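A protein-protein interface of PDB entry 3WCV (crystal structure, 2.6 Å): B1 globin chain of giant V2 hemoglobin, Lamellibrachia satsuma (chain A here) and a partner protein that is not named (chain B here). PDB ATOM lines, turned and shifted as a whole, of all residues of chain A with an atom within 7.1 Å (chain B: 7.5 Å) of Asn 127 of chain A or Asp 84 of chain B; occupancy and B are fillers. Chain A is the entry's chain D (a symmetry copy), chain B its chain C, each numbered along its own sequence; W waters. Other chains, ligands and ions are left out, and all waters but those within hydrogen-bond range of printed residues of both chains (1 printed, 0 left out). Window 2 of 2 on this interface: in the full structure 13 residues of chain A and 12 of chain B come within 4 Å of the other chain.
NH2 of Arg 10 of chain B is in salt-bridge range of OD1 of Asp 131 of chain A (3.1 Å). The side-chain hydroxyl (OG) of Ser 86 of chain B is in hydrogen-bond range of the backbone carbonyl oxygen (O) of Phe 128 of chain A, 3.0 Å away.
Hydrophobic or aromatic side chains of chain B within 4 Å of the printed part of chain A: Pro 85. Of the 12 printed residues of chain A, 5 touch a printed residue of chain B. Printed residues of chain A that touch a printed residue of chain B: Asn 127, Phe 128, Asn 129, Pro 130 and Asp 131.
The backbone carbonyl oxygen (O) of Leu 82 of chain B sits at hydrogen-bond distance from the guanidinium group (NH1) of Arg 10 of chain B (2.9 Å). OD2 of Asp 84 of chain B sits at hydrogen-bond distance from OG1 of Thr 87 of chain B (2.6 Å). The backbone carbonyl oxygen (O) of Pro 85 of chain B lies close to the side-chain amide nitrogen (ND2) of Asn 89 of chain B. The side-chain amide nitrogen (NE2) of Gln 15 of chain A sits at hydrogen-bond distance from the backbone carbonyl oxygen (O) of Asn 127 of chain A (2.7 Å). The backbone NH (N) of Asn 129 of chain A is in hydrogen-bond range of the side-chain amide oxygen (OE1) of Gln 15 of chain A (3.0 Å). The side-chain amide oxygen (OD1) of Asn 129 of chain A sits at hydrogen-bond distance from the backbone NH (N) of Asp 131 of chain A, 2.9 Å away.
Asp 84 of chain B touches Asn 127 of chain A. CG of Pro 85 of chain B touches OD1 of Asn 129 of chain A, at 2.8 Å. Pro 130 of chain A touches Pro 85 of chain B (CG to CB, 3.8 Å). CD of Pro 130 of chain A touches OG of Ser 86 of chain B, 3.7 Å away. Pro 130 of chain A touches Asn 89 of chain B (CG to ND2, 3.6 Å). CG of Asp 131 of chain A touches CB of Pro 85 of chain B (3.5 Å).
Gln 18 of chain A touches none of the printed residues of chain B. Printed residues of chain B within 4 Å of Phe 128 of chain A: Ser 86. Of the printed residues of chain B, Pro 130 of chain A touches Pro 85 (3.8 Å), Ser 86 (3.7 Å) and Asn 89 (3.6 Å). Printed residues of chain B within 4 Å of Asp 131 of chain A: Arg 10 and Pro 85. Asp 84 of chain B touches one residue of chain A. Of the printed residues of chain A, Ser 86 of chain B touches Phe 128 (3.0 Å) and Pro 130 (3.7 Å). Of the printed residues of chain A, Asn 89 of chain B touches Pro 130.
Water W1 lies within hydrogen-bond range of the side-chain carboxylate of Asp 84 of chain B (2.7 Å), the backbone NH of Ser 86 of chain B (2.8 Å) and the backbone carbonyl oxygen of Phe 128 of chain A (3.1 Å).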
ATOM      1  N   ILE A  11     -21.847 -20.562  -3.517  1.00  0.00           N
ATOM      2  CA  ILE A  11     -20.714 -20.423  -4.415  1.00  0.00           C
ATOM      3  C   ILE A  11     -19.452 -20.941  -3.771  1.00  0.00           C
ATOM      4  O   ILE A  11     -18.687 -21.688  -4.395  1.00  0.00           O
ATOM      5  CB  ILE A  11     -20.497 -18.966  -4.827  1.00  0.00           C
ATOM      6  CG1 ILE A  11     -21.704 -18.479  -5.635  1.00  0.00           C
ATOM      7  CG2 ILE A  11     -19.180 -18.839  -5.626  1.00  0.00           C
ATOM      8  CD1 ILE A  11     -21.607 -17.036  -6.038  1.00  0.00           C
ATOM      9  N   GLN A  15     -17.124 -23.929  -5.243  1.00  0.00           N
ATOM     10  CA  GLN A  15     -15.745 -23.748  -5.687  1.00  0.00           C
ATOM     11  C   GLN A  15     -14.788 -24.586  -4.861  1.00  0.00           C
ATOM     12  O   GLN A  15     -13.837 -25.159  -5.399  1.00  0.00           O
ATOM     13  CB  GLN A  15     -15.315 -22.278  -5.620  1.00  0.00           C
ATOM     14  CG  GLN A  15     -16.206 -21.325  -6.415  1.00  0.00           C
ATOM     15  CD  GLN A  15     -15.540 -19.988  -6.686  1.00  0.00           C
ATOM     16  OE1 GLN A  15     -14.984 -19.365  -5.792  1.00  0.00           O
ATOM     17  NE2 GLN A  15     -15.604 -19.542  -7.922  1.00  0.00           N
ATOM     18  N   GLN A  18     -14.572 -28.172  -5.657  1.00  0.00           N
ATOM     19  CA  GLN A  18     -13.890 -28.357  -6.936  1.00  0.00           C
ATOM     20  C   GLN A  18     -12.527 -28.957  -6.672  1.00  0.00           C
ATOM     21  O   GLN A  18     -12.100 -29.897  -7.336  1.00  0.00           O
ATOM     22  CB  GLN A  18     -13.641 -27.016  -7.613  1.00  0.00           C
ATOM     23  CG  GLN A  18     -14.525 -26.656  -8.761  1.00  0.00           C
ATOM     24  CD  GLN A  18     -14.056 -25.377  -9.413  1.00  0.00           C
ATOM     25  OE1 GLN A  18     -12.921 -25.288  -9.893  1.00  0.00           O
ATOM     26  NE2 GLN A  18     -14.924 -24.369  -9.424  1.00  0.00           N
ATOM     27  N   PRO A 122      -7.273 -18.908  -5.763  1.00  0.00           N
ATOM     28  CA  PRO A 122      -7.486 -18.571  -7.179  1.00  0.00           C
ATOM     29  C   PRO A 122      -6.622 -19.356  -8.164  1.00  0.00           C
ATOM     30  O   PRO A 122      -6.974 -19.480  -9.335  1.00  0.00           O
ATOM     31  CB  PRO A 122      -7.229 -17.066  -7.228  1.00  0.00           C
ATOM     32  CG  PRO A 122      -6.416 -16.802  -6.010  1.00  0.00           C
ATOM     33  CD  PRO A 122      -7.005 -17.699  -4.978  1.00  0.00           C
ATOM     34  N   ILE A 125      -8.727 -22.863  -8.081  1.00  0.00           N
ATOM     35  CA  ILE A 125     -10.147 -22.814  -8.414  1.00  0.00           C
ATOM     36  C   ILE A 125     -10.546 -22.066  -9.695  1.00  0.00           C
ATOM     37  O   ILE A 125     -10.051 -20.971  -9.963  1.00  0.00           O
ATOM     38  CB  ILE A 125     -10.915 -22.216  -7.196  1.00  0.00           C
ATOM     39  CG1 ILE A 125     -10.802 -23.170  -6.005  1.00  0.00           C
ATOM     40  CG2 ILE A 125     -12.366 -21.937  -7.540  1.00  0.00           C
ATOM     41  CD1 ILE A 125     -11.257 -22.565  -4.678  1.00  0.00           C
ATOM     42  N   ASP A 126     -11.469 -22.663 -10.459  1.00  0.00           N
ATOM     43  CA  ASP A 126     -11.969 -22.065 -11.697  1.00  0.00           C
ATOM     44  C   ASP A 126     -12.838 -20.858 -11.369  1.00  0.00           C
ATOM     45  O   ASP A 126     -13.798 -20.972 -10.612  1.00  0.00           O
ATOM     46  CB  ASP A 126     -12.806 -23.063 -12.499  1.00  0.00           C
ATOM     47  CG  ASP A 126     -11.977 -24.172 -13.102  1.00  0.00           C
ATOM     48  OD1 ASP A 126     -10.760 -23.975 -13.299  1.00  0.00           O
ATOM     49  OD2 ASP A 126     -12.551 -25.249 -13.398  1.00  0.00           O
ATOM     50  N   ASN A 127     -12.509 -19.710 -11.952  1.00  0.00           N
ATOM     51  CA  ASN A 127     -13.254 -18.475 -11.697  1.00  0.00           C
ATOM     52  C   ASN A 127     -13.467 -18.191 -10.235  1.00  0.00           C
ATOM     53  O   ASN A 127     -14.570 -17.874  -9.814  1.00  0.00           O
ATOM     54  CB  ASN A 127     -14.615 -18.496 -12.388  1.00  0.00           C
ATOM     55  CG  ASN A 127     -14.559 -17.936 -13.784  1.00  0.00           C
ATOM     56  OD1 ASN A 127     -14.275 -16.754 -13.993  1.00  0.00           O
ATOM     57  ND2 ASN A 127     -14.820 -18.789 -14.758  1.00  0.00           N
ATOM     58  N   PHE A 128     -12.401 -18.313  -9.459  1.00  0.00           N
ATOM     59  CA  PHE A 128     -12.463 -18.030  -8.034  1.00  0.00           C
ATOM     60  C   PHE A 128     -13.201 -16.709  -7.802  1.00  0.00           C
ATOM     61  O   PHE A 128     -12.964 -15.723  -8.509  1.00  0.00           O
ATOM     62  CB  PHE A 128     -11.039 -17.918  -7.483  1.00  0.00           C
ATOM     63  CG  PHE A 128     -10.978 -17.513  -6.037  1.00  0.00           C
ATOM     64  CD1 PHE A 128     -11.206 -18.443  -5.030  1.00  0.00           C
ATOM     65  CD2 PHE A 128     -10.673 -16.204  -5.684  1.00  0.00           C
ATOM     66  CE1 PHE A 128     -11.125 -18.077  -3.713  1.00  0.00           C
ATOM     67  CE2 PHE A 128     -10.596 -15.840  -4.368  1.00  0.00           C
ATOM     68  CZ  PHE A 128     -10.819 -16.778  -3.378  1.00  0.00           C
ATOM     69  N   ASN A 129     -14.076 -16.678  -6.806  1.00  0.00           N
ATOM     70  CA  ASN A 129     -14.808 -15.455  -6.502  1.00  0.00           C
ATOM     71  C   ASN A 129     -14.367 -14.849  -5.174  1.00  0.00           C
ATOM     72  O   ASN A 129     -14.856 -15.229  -4.115  1.00  0.00           O
ATOM     73  CB  ASN A 129     -16.293 -15.736  -6.446  1.00  0.00           C
ATOM     74  CG  ASN A 129     -17.102 -14.487  -6.225  1.00  0.00           C
ATOM     75  OD1 ASN A 129     -16.701 -13.583  -5.474  1.00  0.00           O
ATOM     76  ND2 ASN A 129     -18.262 -14.429  -6.866  1.00  0.00           N
ATOM     77  N   PRO A 130     -13.442 -13.878  -5.217  1.00  0.00           N
ATOM     78  CA  PRO A 130     -12.937 -13.223  -4.004  1.00  0.00           C
ATOM     79  C   PRO A 130     -13.976 -12.607  -3.073  1.00  0.00           C
ATOM     80  O   PRO A 130     -13.837 -12.645  -1.849  1.00  0.00           O
ATOM     81  CB  PRO A 130     -11.977 -12.179  -4.562  1.00  0.00           C
ATOM     82  CG  PRO A 130     -12.561 -11.889  -5.926  1.00  0.00           C
ATOM     83  CD  PRO A 130     -12.878 -13.250  -6.426  1.00  0.00           C
ATOM     84  N   ASP A 131     -15.021 -12.031  -3.644  1.00  0.00           N
ATOM     85  CA  ASP A 131     -16.044 -11.423  -2.813  1.00  0.00           C
ATOM     86  C   ASP A 131     -16.858 -12.454  -2.049  1.00  0.00           C
ATOM     87  O   ASP A 131     -17.018 -12.356  -0.827  1.00  0.00           O
ATOM     88  CB  ASP A 131     -16.966 -10.543  -3.658  1.00  0.00           C
ATOM     89  CG  ASP A 131     -16.296  -9.232  -4.078  1.00  0.00           C
ATOM     90  OD1 ASP A 131     -16.982  -8.361  -4.658  1.00  0.00           O
ATOM     91  OD2 ASP A 131     -15.078  -9.075  -3.822  1.00  0.00           O
ATOM     92  N   TRP A 133     -16.050 -15.337  -1.299  1.00  0.00           N
ATOM     93  CA  TRP A 133     -15.185 -15.979  -0.325  1.00  0.00           C
ATOM     94  C   TRP A 133     -14.960 -15.059   0.869  1.00  0.00           C
ATOM     95  O   TRP A 133     -15.072 -15.494   2.012  1.00  0.00           O
ATOM     96  CB  TRP A 133     -13.852 -16.400  -0.958  1.00  0.00           C
ATOM     97  CG  TRP A 133     -13.914 -17.731  -1.651  1.00  0.00           C
ATOM     98  CD1 TRP A 133     -14.275 -17.959  -2.942  1.00  0.00           C
ATOM     99  CD2 TRP A 133     -13.610 -19.017  -1.085  1.00  0.00           C
ATOM    100  NE1 TRP A 133     -14.211 -19.306  -3.225  1.00  0.00           N
ATOM    101  CE2 TRP A 133     -13.804 -19.980  -2.104  1.00  0.00           C
ATOM    102  CE3 TRP A 133     -13.193 -19.448   0.184  1.00  0.00           C
ATOM    103  CZ2 TRP A 133     -13.597 -21.349  -1.901  1.00  0.00           C
ATOM    104  CZ3 TRP A 133     -12.985 -20.822   0.391  1.00  0.00           C
ATOM    105  CH2 TRP A 133     -13.190 -21.753  -0.655  1.00  0.00           C
ATOM    106  N   ARG B  10     -26.593  -8.366  -5.539  1.00  0.00           N
ATOM    107  CA  ARG B  10     -26.020  -8.081  -6.847  1.00  0.00           C
ATOM    108  C   ARG B  10     -27.023  -8.366  -7.950  1.00  0.00           C
ATOM    109  O   ARG B  10     -27.166  -7.567  -8.870  1.00  0.00           O
ATOM    110  CB  ARG B  10     -24.758  -8.918  -7.056  1.00  0.00           C
ATOM    111  CG  ARG B  10     -23.643  -8.498  -6.129  1.00  0.00           C
ATOM    112  CD  ARG B  10     -22.559  -9.552  -5.950  1.00  0.00           C
ATOM    113  NE  ARG B  10     -21.779  -9.222  -4.757  1.00  0.00           N
ATOM    114  CZ  ARG B  10     -20.488  -8.897  -4.756  1.00  0.00           C
ATOM    115  NH1 ARG B  10     -19.814  -8.873  -5.901  1.00  0.00           N
ATOM    116  NH2 ARG B  10     -19.891  -8.562  -3.612  1.00  0.00           N
ATOM    117  N   GLN B  14     -28.375  -5.397 -10.374  1.00  0.00           N
ATOM    118  CA  GLN B  14     -28.317  -5.476 -11.826  1.00  0.00           C
ATOM    119  C   GLN B  14     -29.738  -5.307 -12.349  1.00  0.00           C
ATOM    120  O   GLN B  14     -29.949  -4.724 -13.450  1.00  0.00           O
ATOM    121  CB  GLN B  14     -27.747  -6.815 -12.245  1.00  0.00           C
ATOM    122  CG  GLN B  14     -26.301  -6.946 -11.863  1.00  0.00           C
ATOM    123  CD  GLN B  14     -25.713  -8.303 -12.182  1.00  0.00           C
ATOM    124  OE1 GLN B  14     -24.503  -8.482 -12.103  1.00  0.00           O
ATOM    125  NE2 GLN B  14     -26.560  -9.273 -12.535  1.00  0.00           N
ATOM    126  N   ALA B  78     -19.130  -1.582 -13.752  1.00  0.00           N
ATOM    127  CA  ALA B  78     -18.924  -2.147 -12.433  1.00  0.00           C
ATOM    128  C   ALA B  78     -20.140  -2.976 -11.979  1.00  0.00           C
ATOM    129  O   ALA B  78     -19.982  -4.062 -11.414  1.00  0.00           O
ATOM    130  CB  ALA B  78     -18.623  -1.025 -11.428  1.00  0.00           C
ATOM    131  N   ILE B  79     -21.350  -2.468 -12.227  1.00  0.00           N
ATOM    132  CA  ILE B  79     -22.561  -3.180 -11.833  1.00  0.00           C
ATOM    133  C   ILE B  79     -22.631  -4.541 -12.520  1.00  0.00           C
ATOM    134  O   ILE B  79     -22.995  -5.555 -11.899  1.00  0.00           O
ATOM    135  CB  ILE B  79     -23.807  -2.338 -12.121  1.00  0.00           C
ATOM    136  CG1 ILE B  79     -23.938  -1.262 -11.037  1.00  0.00           C
ATOM    137  CG2 ILE B  79     -25.047  -3.212 -12.127  1.00  0.00           C
ATOM    138  CD1 ILE B  79     -24.978  -0.250 -11.288  1.00  0.00           C
ATOM    139  N   GLY B  80     -22.254  -4.566 -13.797  1.00  0.00           N
ATOM    140  CA  GLY B  80     -22.245  -5.816 -14.518  1.00  0.00           C
ATOM    141  C   GLY B  80     -21.196  -6.747 -13.913  1.00  0.00           C
ATOM    142  O   GLY B  80     -21.464  -7.932 -13.679  1.00  0.00           O
ATOM    143  N   LEU B  81     -20.005  -6.212 -13.630  1.00  0.00           N
ATOM    144  CA  LEU B  81     -18.921  -7.020 -13.078  1.00  0.00           C
ATOM    145  C   LEU B  81     -19.090  -7.486 -11.619  1.00  0.00           C
ATOM    146  O   LEU B  81     -18.225  -8.185 -11.087  1.00  0.00           O
ATOM    147  CB  LEU B  81     -17.579  -6.295 -13.278  1.00  0.00           C
ATOM    148  CG  LEU B  81     -17.111  -6.237 -14.754  1.00  0.00           C
ATOM    149  CD1 LEU B  81     -15.892  -5.365 -14.884  1.00  0.00           C
ATOM    150  CD2 LEU B  81     -16.801  -7.634 -15.270  1.00  0.00           C
ATOM    151  N   LEU B  82     -20.199  -7.129 -10.975  1.00  0.00           N
ATOM    152  CA  LEU B  82     -20.428  -7.588  -9.603  1.00  0.00           C
ATOM    153  C   LEU B  82     -20.505  -9.118  -9.645  1.00  0.00           C
ATOM    154  O   LEU B  82     -20.258  -9.785  -8.647  1.00  0.00           O
ATOM    155  CB  LEU B  82     -21.733  -7.007  -9.040  1.00  0.00           C
ATOM    156  CG  LEU B  82     -21.708  -5.550  -8.557  1.00  0.00           C
ATOM    157  CD1 LEU B  82     -23.104  -5.031  -8.286  1.00  0.00           C
ATOM    158  CD2 LEU B  82     -20.877  -5.470  -7.283  1.00  0.00           C
ATOM    159  N   SER B  83     -20.835  -9.649 -10.825  1.00  0.00           N
ATOM    160  CA  SER B  83     -20.966 -11.089 -11.077  1.00  0.00           C
ATOM    161  C   SER B  83     -19.652 -11.834 -11.246  1.00  0.00           C
ATOM    162  O   SER B  83     -19.620 -13.063 -11.209  1.00  0.00           O
ATOM    163  CB  SER B  83     -21.795 -11.327 -12.334  1.00  0.00           C
ATOM    164  OG  SER B  83     -23.071 -10.734 -12.210  1.00  0.00           O
ATOM    165  N   ASP B  84     -18.581 -11.086 -11.484  1.00  0.00           N
ATOM    166  CA  ASP B  84     -17.256 -11.654 -11.652  1.00  0.00           C
ATOM    167  C   ASP B  84     -16.278 -10.726 -10.937  1.00  0.00           C
ATOM    168  O   ASP B  84     -15.534  -9.969 -11.567  1.00  0.00           O
ATOM    169  CB  ASP B  84     -16.914 -11.771 -13.141  1.00  0.00           C
ATOM    170  CG  ASP B  84     -15.495 -12.289 -13.377  1.00  0.00           C
ATOM    171  OD1 ASP B  84     -15.034 -13.153 -12.591  1.00  0.00           O
ATOM    172  OD2 ASP B  84     -14.835 -11.855 -14.354  1.00  0.00           O
ATOM    173  N   PRO B  85     -16.286 -10.769  -9.589  1.00  0.00           N
ATOM    174  CA  PRO B  85     -15.414  -9.945  -8.759  1.00  0.00           C
ATOM    175  C   PRO B  85     -13.909  -9.941  -9.075  1.00  0.00           C
ATOM    176  O   PRO B  85     -13.259  -8.921  -8.849  1.00  0.00           O
ATOM    177  CB  PRO B  85     -15.744 -10.428  -7.341  1.00  0.00           C
ATOM    178  CG  PRO B  85     -16.325 -11.764  -7.548  1.00  0.00           C
ATOM    179  CD  PRO B  85     -17.170 -11.579  -8.742  1.00  0.00           C
ATOM    180  N   SER B  86     -13.349 -11.043  -9.581  1.00  0.00           N
ATOM    181  CA  SER B  86     -11.913 -11.059  -9.932  1.00  0.00           C
ATOM    182  C   SER B  86     -11.615  -9.884 -10.862  1.00  0.00           C
ATOM    183  O   SER B  86     -10.741  -9.058 -10.600  1.00  0.00           O
ATOM    184  CB  SER B  86     -11.513 -12.347 -10.660  1.00  0.00           C
ATOM    185  OG  SER B  86     -11.454 -13.453  -9.781  1.00  0.00           O
ATOM    186  N   THR B  87     -12.362  -9.827 -11.955  1.00  0.00           N
ATOM    187  CA  THR B  87     -12.218  -8.773 -12.940  1.00  0.00           C
ATOM    188  C   THR B  87     -12.730  -7.449 -12.372  1.00  0.00           C
ATOM    189  O   THR B  87     -12.184  -6.390 -12.667  1.00  0.00           O
ATOM    190  CB  THR B  87     -12.996  -9.130 -14.204  1.00  0.00           C
ATOM    191  OG1 THR B  87     -12.621 -10.452 -14.622  1.00  0.00           O
ATOM    192  CG2 THR B  87     -12.709  -8.133 -15.307  1.00  0.00           C
ATOM    193  N   LEU B  88     -13.775  -7.503 -11.554  1.00  0.00           N
ATOM    194  CA  LEU B  88     -14.294  -6.280 -10.960  1.00  0.00           C
ATOM    195  C   LEU B  88     -13.131  -5.573 -10.268  1.00  0.00           C
ATOM    196  O   LEU B  88     -12.909  -4.383 -10.482  1.00  0.00           O
ATOM    197  CB  LEU B  88     -15.397  -6.582  -9.923  1.00  0.00           C
ATOM    198  CG  LEU B  88     -15.859  -5.395  -9.050  1.00  0.00           C
ATOM    199  CD1 LEU B  88     -16.664  -4.412  -9.892  1.00  0.00           C
ATOM    200  CD2 LEU B  88     -16.702  -5.883  -7.893  1.00  0.00           C
ATOM    201  N   ASN B  89     -12.387  -6.324  -9.452  1.00  0.00           N
ATOM    202  CA  ASN B  89     -11.256  -5.768  -8.710  1.00  0.00           C
ATOM    203  C   ASN B  89     -10.293  -5.008  -9.593  1.00  0.00           C
ATOM    204  O   ASN B  89      -9.853  -3.923  -9.232  1.00  0.00           O
ATOM    205  CB  ASN B  89     -10.500  -6.861  -7.960  1.00  0.00           C
ATOM    206  CG  ASN B  89     -11.268  -7.374  -6.773  1.00  0.00           C
ATOM    207  OD1 ASN B  89     -12.079  -6.643  -6.193  1.00  0.00           O
ATOM    208  ND2 ASN B  89     -11.018  -8.638  -6.386  1.00  0.00           N
ATOM    209  N   GLU B  90      -9.963  -5.583 -10.744  1.00  0.00           N
ATOM    210  CA  GLU B  90      -9.061  -4.940 -11.680  1.00  0.00           C
ATOM    211  C   GLU B  90      -9.685  -3.644 -12.188  1.00  0.00           C
ATOM    212  O   GLU B  90      -9.035  -2.605 -12.228  1.00  0.00           O
ATOM    213  CB  GLU B  90      -8.742  -5.891 -12.836  1.00  0.00           C
ATOM    214  CG  GLU B  90      -7.865  -7.064 -12.425  1.00  0.00           C
ATOM    215  CD  GLU B  90      -6.613  -6.614 -11.667  1.00  0.00           C
ATOM    216  OE1 GLU B  90      -5.784  -5.882 -12.258  1.00  0.00           O
ATOM    217  OE2 GLU B  90      -6.463  -6.987 -10.473  1.00  0.00           O
HETATM  218  O   HOH W   1     -14.627 -13.473  -9.923  1.00  0.00           O
